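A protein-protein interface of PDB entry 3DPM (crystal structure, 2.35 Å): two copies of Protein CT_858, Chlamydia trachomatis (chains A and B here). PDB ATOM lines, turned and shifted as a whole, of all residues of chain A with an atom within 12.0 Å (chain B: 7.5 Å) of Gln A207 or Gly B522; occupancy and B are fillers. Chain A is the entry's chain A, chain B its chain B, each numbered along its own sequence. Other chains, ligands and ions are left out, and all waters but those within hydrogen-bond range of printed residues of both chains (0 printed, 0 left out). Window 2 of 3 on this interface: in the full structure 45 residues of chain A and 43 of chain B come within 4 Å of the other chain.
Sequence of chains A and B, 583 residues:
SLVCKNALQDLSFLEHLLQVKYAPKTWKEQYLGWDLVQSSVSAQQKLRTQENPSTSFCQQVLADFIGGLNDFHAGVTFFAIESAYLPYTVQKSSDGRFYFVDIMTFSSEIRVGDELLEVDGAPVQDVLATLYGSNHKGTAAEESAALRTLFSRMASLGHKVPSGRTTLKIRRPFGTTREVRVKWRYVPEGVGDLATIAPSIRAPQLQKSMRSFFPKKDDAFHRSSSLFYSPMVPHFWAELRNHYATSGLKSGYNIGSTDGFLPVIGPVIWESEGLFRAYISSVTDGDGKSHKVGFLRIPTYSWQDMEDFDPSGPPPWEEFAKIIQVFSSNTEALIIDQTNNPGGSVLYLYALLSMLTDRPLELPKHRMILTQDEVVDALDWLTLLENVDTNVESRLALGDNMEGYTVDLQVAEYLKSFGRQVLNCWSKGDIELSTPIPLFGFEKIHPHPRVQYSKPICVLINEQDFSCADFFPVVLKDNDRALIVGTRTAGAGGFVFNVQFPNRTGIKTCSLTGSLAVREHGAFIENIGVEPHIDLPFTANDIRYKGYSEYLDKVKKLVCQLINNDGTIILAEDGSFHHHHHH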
ATOM      1  N   ALA A 203      33.570 -20.622  28.367  1.00  0.00           N
ATOM      2  CA  ALA A 203      32.488 -20.733  29.335  1.00  0.00           C
ATOM      3  C   ALA A 203      31.252 -20.001  28.808  1.00  0.00           C
ATOM      4  O   ALA A 203      31.365 -19.018  28.070  1.00  0.00           O
ATOM      5  CB  ALA A 203      32.920 -20.141  30.675  1.00  0.00           C
ATOM      6  N   PRO A 204      30.054 -20.478  29.176  1.00  0.00           N
ATOM      7  CA  PRO A 204      28.813 -19.842  28.723  1.00  0.00           C
ATOM      8  C   PRO A 204      28.668 -18.388  29.184  1.00  0.00           C
ATOM      9  O   PRO A 204      28.827 -18.082  30.363  1.00  0.00           O
ATOM     10  CB  PRO A 204      27.723 -20.764  29.287  1.00  0.00           C
ATOM     11  CG  PRO A 204      28.376 -21.384  30.491  1.00  0.00           C
ATOM     12  CD  PRO A 204      29.773 -21.659  30.012  1.00  0.00           C
ATOM     13  N   GLN A 205      28.372 -17.506  28.232  1.00  0.00           N
ATOM     14  CA  GLN A 205      28.199 -16.074  28.476  1.00  0.00           C
ATOM     15  C   GLN A 205      26.856 -15.631  27.907  1.00  0.00           C
ATOM     16  O   GLN A 205      26.523 -15.976  26.774  1.00  0.00           O
ATOM     17  CB  GLN A 205      29.321 -15.301  27.788  1.00  0.00           C
ATOM     18  CG  GLN A 205      30.663 -15.391  28.489  1.00  0.00           C
ATOM     19  CD  GLN A 205      30.913 -14.199  29.401  1.00  0.00           C
ATOM     20  OE1 GLN A 205      31.039 -13.065  28.934  1.00  0.00           O
ATOM     21  NE2 GLN A 205      30.980 -14.449  30.709  1.00  0.00           N
ATOM     22  N   LEU A 206      26.091 -14.854  28.671  1.00  0.00           N
ATOM     23  CA  LEU A 206      24.775 -14.403  28.212  1.00  0.00           C
ATOM     24  C   LEU A 206      24.754 -13.273  27.176  1.00  0.00           C
ATOM     25  O   LEU A 206      25.640 -12.417  27.154  1.00  0.00           O
ATOM     26  CB  LEU A 206      23.905 -14.021  29.414  1.00  0.00           C
ATOM     27  CG  LEU A 206      23.402 -15.203  30.250  1.00  0.00           C
ATOM     28  CD1 LEU A 206      22.505 -14.712  31.369  1.00  0.00           C
ATOM     29  CD2 LEU A 206      22.643 -16.162  29.359  1.00  0.00           C
ATOM     30  N   GLN A 207      23.722 -13.296  26.325  1.00  0.00           N
ATOM     31  CA  GLN A 207      23.496 -12.320  25.243  1.00  0.00           C
ATOM     32  C   GLN A 207      24.728 -11.510  24.835  1.00  0.00           C
ATOM     33  O   GLN A 207      24.648 -10.624  23.978  1.00  0.00           O
ATOM     34  CB  GLN A 207      22.353 -11.354  25.613  1.00  0.00           C
ATOM     35  CG  GLN A 207      22.723 -10.289  26.646  1.00  0.00           C
ATOM     36  CD  GLN A 207      21.540  -9.420  27.058  1.00  0.00           C
ATOM     37  OE1 GLN A 207      21.705  -8.426  27.768  1.00  0.00           O
ATOM     38  NE2 GLN A 207      20.343  -9.794  26.622  1.00  0.00           N
ATOM     39  N   TRP B  27      20.848 -18.623  32.191  1.00  0.00           N
ATOM     40  CA  TRP B  27      19.768 -17.650  32.253  1.00  0.00           C
ATOM     41  C   TRP B  27      18.976 -17.798  33.551  1.00  0.00           C
ATOM     42  O   TRP B  27      18.631 -16.807  34.193  1.00  0.00           O
ATOM     43  CB  TRP B  27      18.837 -17.821  31.047  1.00  0.00           C
ATOM     44  CG  TRP B  27      17.554 -17.063  31.158  1.00  0.00           C
ATOM     45  CD1 TRP B  27      16.301 -17.587  31.309  1.00  0.00           C
ATOM     46  CD2 TRP B  27      17.391 -15.642  31.111  1.00  0.00           C
ATOM     47  NE1 TRP B  27      15.368 -16.580  31.351  1.00  0.00           N
ATOM     48  CE2 TRP B  27      16.010 -15.376  31.233  1.00  0.00           C
ATOM     49  CE3 TRP B  27      18.281 -14.566  30.982  1.00  0.00           C
ATOM     50  CZ2 TRP B  27      15.494 -14.075  31.224  1.00  0.00           C
ATOM     51  CZ3 TRP B  27      17.767 -13.269  30.975  1.00  0.00           C
ATOM     52  CH2 TRP B  27      16.385 -13.039  31.095  1.00  0.00           C
ATOM     53  N   ARG B 367      20.604 -19.678  20.891  1.00  0.00           N
ATOM     54  CA  ARG B 367      21.913 -19.964  21.486  1.00  0.00           C
ATOM     55  C   ARG B 367      21.801 -21.454  21.835  1.00  0.00           C
ATOM     56  O   ARG B 367      20.919 -21.839  22.608  1.00  0.00           O
ATOM     57  CB  ARG B 367      22.121 -19.163  22.779  1.00  0.00           C
ATOM     58  CG  ARG B 367      21.963 -17.640  22.682  1.00  0.00           C
ATOM     59  CD  ARG B 367      23.164 -16.951  22.058  1.00  0.00           C
ATOM     60  NE  ARG B 367      24.443 -17.301  22.696  1.00  0.00           N
ATOM     61  CZ  ARG B 367      24.870 -16.850  23.874  1.00  0.00           C
ATOM     62  NH1 ARG B 367      24.130 -16.010  24.577  1.00  0.00           N
ATOM     63  NH2 ARG B 367      26.045 -17.248  24.353  1.00  0.00           N
ATOM     64  N   LEU B 433      27.255 -22.587  24.976  1.00  0.00           N
ATOM     65  CA  LEU B 433      26.065 -21.773  24.723  1.00  0.00           C
ATOM     66  C   LEU B 433      26.435 -20.975  23.482  1.00  0.00           C
ATOM     67  O   LEU B 433      26.799 -19.805  23.558  1.00  0.00           O
ATOM     68  CB  LEU B 433      25.761 -20.839  25.893  1.00  0.00           C
ATOM     69  CG  LEU B 433      24.423 -20.095  25.773  1.00  0.00           C
ATOM     70  CD1 LEU B 433      23.286 -21.112  25.671  1.00  0.00           C
ATOM     71  CD2 LEU B 433      24.216 -19.181  26.970  1.00  0.00           C
ATOM     72  N   PRO B 436      24.293 -17.057  18.611  1.00  0.00           N
ATOM     73  CA  PRO B 436      22.948 -17.366  18.107  1.00  0.00           C
ATOM     74  C   PRO B 436      22.914 -17.989  16.712  1.00  0.00           C
ATOM     75  O   PRO B 436      23.588 -17.533  15.785  1.00  0.00           O
ATOM     76  CB  PRO B 436      22.212 -16.025  18.199  1.00  0.00           C
ATOM     77  CG  PRO B 436      23.312 -14.999  18.270  1.00  0.00           C
ATOM     78  CD  PRO B 436      24.380 -15.666  19.085  1.00  0.00           C
ATOM     79  N   ASP B 478       8.143  -7.788  15.983  1.00  0.00           N
ATOM     80  CA  ASP B 478       9.464  -7.248  15.684  1.00  0.00           C
ATOM     81  C   ASP B 478       9.672  -6.759  14.256  1.00  0.00           C
ATOM     82  O   ASP B 478      10.581  -5.966  14.003  1.00  0.00           O
ATOM     83  CB  ASP B 478      10.545  -8.272  16.030  1.00  0.00           C
ATOM     84  CG  ASP B 478      10.699  -8.474  17.530  1.00  0.00           C
ATOM     85  OD1 ASP B 478      10.000  -7.774  18.308  1.00  0.00           O
ATOM     86  OD2 ASP B 478      11.525  -9.335  17.926  1.00  0.00           O
ATOM     87  N   LEU B 516      18.203 -21.412  23.736  1.00  0.00           N
ATOM     88  CA  LEU B 516      17.733 -20.176  24.351  1.00  0.00           C
ATOM     89  C   LEU B 516      17.466 -19.230  23.186  1.00  0.00           C
ATOM     90  O   LEU B 516      18.409 -18.747  22.563  1.00  0.00           O
ATOM     91  CB  LEU B 516      18.837 -19.577  25.225  1.00  0.00           C
ATOM     92  CG  LEU B 516      18.640 -19.221  26.697  1.00  0.00           C
ATOM     93  CD1 LEU B 516      19.451 -17.953  26.958  1.00  0.00           C
ATOM     94  CD2 LEU B 516      17.178 -18.984  27.040  1.00  0.00           C
ATOM     95  N   ALA B 517      16.198 -18.985  22.871  1.00  0.00           N
ATOM     96  CA  ALA B 517      15.858 -18.083  21.767  1.00  0.00           C
ATOM     97  C   ALA B 517      16.186 -16.635  22.143  1.00  0.00           C
ATOM     98  O   ALA B 517      16.065 -16.244  23.301  1.00  0.00           O
ATOM     99  CB  ALA B 517      14.371 -18.211  21.411  1.00  0.00           C
ATOM    100  N   VAL B 518      16.612 -15.857  21.153  1.00  0.00           N
ATOM    101  CA  VAL B 518      16.960 -14.453  21.336  1.00  0.00           C
ATOM    102  C   VAL B 518      16.333 -13.669  20.184  1.00  0.00           C
ATOM    103  O   VAL B 518      16.396 -14.097  19.037  1.00  0.00           O
ATOM    104  CB  VAL B 518      18.500 -14.231  21.295  1.00  0.00           C
ATOM    105  CG1 VAL B 518      18.826 -12.765  21.542  1.00  0.00           C
ATOM    106  CG2 VAL B 518      19.182 -15.089  22.350  1.00  0.00           C
ATOM    107  N   ARG B 519      15.729 -12.526  20.494  1.00  0.00           N
ATOM    108  CA  ARG B 519      15.087 -11.697  19.475  1.00  0.00           C
ATOM    109  C   ARG B 519      16.081 -10.765  18.782  1.00  0.00           C
ATOM    110  O   ARG B 519      17.178 -10.524  19.290  1.00  0.00           O
ATOM    111  CB  ARG B 519      13.966 -10.886  20.119  1.00  0.00           C
ATOM    112  CG  ARG B 519      12.921 -11.765  20.781  1.00  0.00           C
ATOM    113  CD  ARG B 519      12.036 -10.986  21.730  1.00  0.00           C
ATOM    114  NE  ARG B 519      11.222  -9.978  21.063  1.00  0.00           N
ATOM    115  CZ  ARG B 519      10.264  -9.290  21.683  1.00  0.00           C
ATOM    116  NH1 ARG B 519      10.021  -9.514  22.965  1.00  0.00           N
ATOM    117  NH2 ARG B 519       9.540  -8.392  21.029  1.00  0.00           N
ATOM    118  N   GLU B 520      15.692 -10.256  17.618  1.00  0.00           N
ATOM    119  CA  GLU B 520      16.544  -9.350  16.842  1.00  0.00           C
ATOM    120  C   GLU B 520      17.355  -8.415  17.732  1.00  0.00           C
ATOM    121  O   GLU B 520      18.584  -8.332  17.620  1.00  0.00           O
ATOM    122  CB  GLU B 520      15.705  -8.465  15.918  1.00  0.00           C
ATOM    123  CG  GLU B 520      15.118  -9.107  14.678  1.00  0.00           C
ATOM    124  CD  GLU B 520      14.497  -8.061  13.761  1.00  0.00           C
ATOM    125  OE1 GLU B 520      15.230  -7.128  13.352  1.00  0.00           O
ATOM    126  OE2 GLU B 520      13.286  -8.162  13.458  1.00  0.00           O
ATOM    127  N   HIS B 521      16.646  -7.722  18.620  1.00  0.00           N
ATOM    128  CA  HIS B 521      17.243  -6.735  19.508  1.00  0.00           C
ATOM    129  C   HIS B 521      17.952  -7.208  20.771  1.00  0.00           C
ATOM    130  O   HIS B 521      18.325  -6.386  21.609  1.00  0.00           O
ATOM    131  CB  HIS B 521      16.181  -5.686  19.856  1.00  0.00           C
ATOM    132  CG  HIS B 521      15.723  -4.885  18.671  1.00  0.00           C
ATOM    133  ND1 HIS B 521      14.609  -4.072  18.699  1.00  0.00           N
ATOM    134  CD2 HIS B 521      16.244  -4.764  17.424  1.00  0.00           C
ATOM    135  CE1 HIS B 521      14.465  -3.485  17.523  1.00  0.00           C
ATOM    136  NE2 HIS B 521      15.444  -3.887  16.731  1.00  0.00           N
ATOM    137  N   GLY B 522      18.147  -8.517  20.915  1.00  0.00           N
ATOM    138  CA  GLY B 522      18.853  -9.022  22.081  1.00  0.00           C
ATOM    139  C   GLY B 522      18.049  -9.654  23.204  1.00  0.00           C
ATOM    140  O   GLY B 522      18.592 -10.447  23.971  1.00  0.00           O
ATOM    141  N   ALA B 523      16.769  -9.313  23.310  1.00  0.00           N
ATOM    142  CA  ALA B 523      15.919  -9.864  24.361  1.00  0.00           C
ATOM    143  C   ALA B 523      15.673 -11.374  24.248  1.00  0.00           C
ATOM    144  O   ALA B 523      15.386 -11.888  23.165  1.00  0.00           O
ATOM    145  CB  ALA B 523      14.570  -9.124  24.383  1.00  0.00           C
ATOM    146  N   PHE B 524      15.786 -12.074  25.374  1.00  0.00           N
ATOM    147  CA  PHE B 524      15.539 -13.506  25.408  1.00  0.00           C
ATOM    148  C   PHE B 524      14.034 -13.687  25.491  1.00  0.00           C
ATOM    149  O   PHE B 524      13.328 -12.802  25.969  1.00  0.00           O
ATOM    150  CB  PHE B 524      16.158 -14.157  26.648  1.00  0.00           C
ATOM    151  CG  PHE B 524      17.658 -14.135  26.671  1.00  0.00           C
ATOM    152  CD1 PHE B 524      18.340 -13.388  27.626  1.00  0.00           C
ATOM    153  CD2 PHE B 524      18.390 -14.867  25.746  1.00  0.00           C
ATOM    154  CE1 PHE B 524      19.727 -13.372  27.658  1.00  0.00           C
ATOM    155  CE2 PHE B 524      19.783 -14.857  25.770  1.00  0.00           C
ATOM    156  CZ  PHE B 524      20.450 -14.108  26.729  1.00  0.00           C
ATOM    157  N   ILE B 525      13.542 -14.832  25.036  1.00  0.00           N
ATOM    158  CA  ILE B 525      12.117 -15.108  25.104  1.00  0.00           C
ATOM    159  C   ILE B 525      11.797 -15.919  26.372  1.00  0.00           C
ATOM    160  O   ILE B 525      10.761 -15.721  27.001  1.00  0.00           O
ATOM    161  CB  ILE B 525      11.645 -15.867  23.838  1.00  0.00           C
ATOM    162  CG1 ILE B 525      11.968 -15.025  22.604  1.00  0.00           C
ATOM    163  CG2 ILE B 525      10.138 -16.123  23.890  1.00  0.00           C
ATOM    164  CD1 ILE B 525      11.565 -15.662  21.295  1.00  0.00           C
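O of Gln A205 is in hydrogen-bond range of NH2 of Arg B367, 2.8 Å away.
O of Gly B522 lies within hydrogen-bond range of NE2 of Gln A207 (3.2 Å).
NH1 of Arg B367 lies close to N of Gln A207.
No position is printed for both chains.
Of the 8 pairs that touch across the chains among the printed residues, none has its exchanged pair printed and touching as well.
Leu B433 touches Pro A204.
CD2 of Leu B433 touches O of Gln A205 (3.95 Å).
Arg B367 touches Leu A206 (NH1 to C, 3.8 Å).
Leu A206 touches Phe B524.
N of Gln A207 touches CZ of Phe B524 (3.4 Å).
Printed residues of chain B within 4 Å of Leu A206: Arg B367 and Phe B524.
Of chain B, only Arg B367 (3.3 Å), Gly B522 (3.2 Å) and Phe B524 (3.4 Å) come within 4 Å of Gln A207.
Trp B27 touches none of the printed residues of chain A.
Printed residues of chain A within 4 Å of Arg B367: Gln A205, Leu A206 and Gln A207.
Of the printed residues of chain A, Leu B433 touches Pro A204 and Gln A205.
Leu B516 touches none of the printed residues of chain A.
Of the printed residues of chain A, Gly B522 touches Gln A207 (3.2 Å).
No residue of chain A comes within 4 Å of Ala B523.
The nearest residue of chain B that does not touch Gln A207 is Ala B523 (4.9 Å).
The nearest printed residue of chain A that does not touch Arg B367 is Pro A204 (5.6 Å).
The guanidinium group (NH2) of Arg B367 is in hydrogen-bond range of the backbone carbonyl oxygen (O) of Leu B433, at 2.8 Å.
The backbone carbonyl oxygen (O) of Leu B516 sits at hydrogen-bond distance from the backbone NH (N) of Arg B367 (2.9 Å).
Printed residues of chain B that touch a printed residue of chain A: Arg B367, Leu B433, Gly B522 and Phe B524.
Among the printed residues, 8 pairs touch across the chains.
Among the printed residues, no Asp or Glu carboxylate lies within 4 Å of a Lys or Arg side-chain nitrogen of the other chain.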
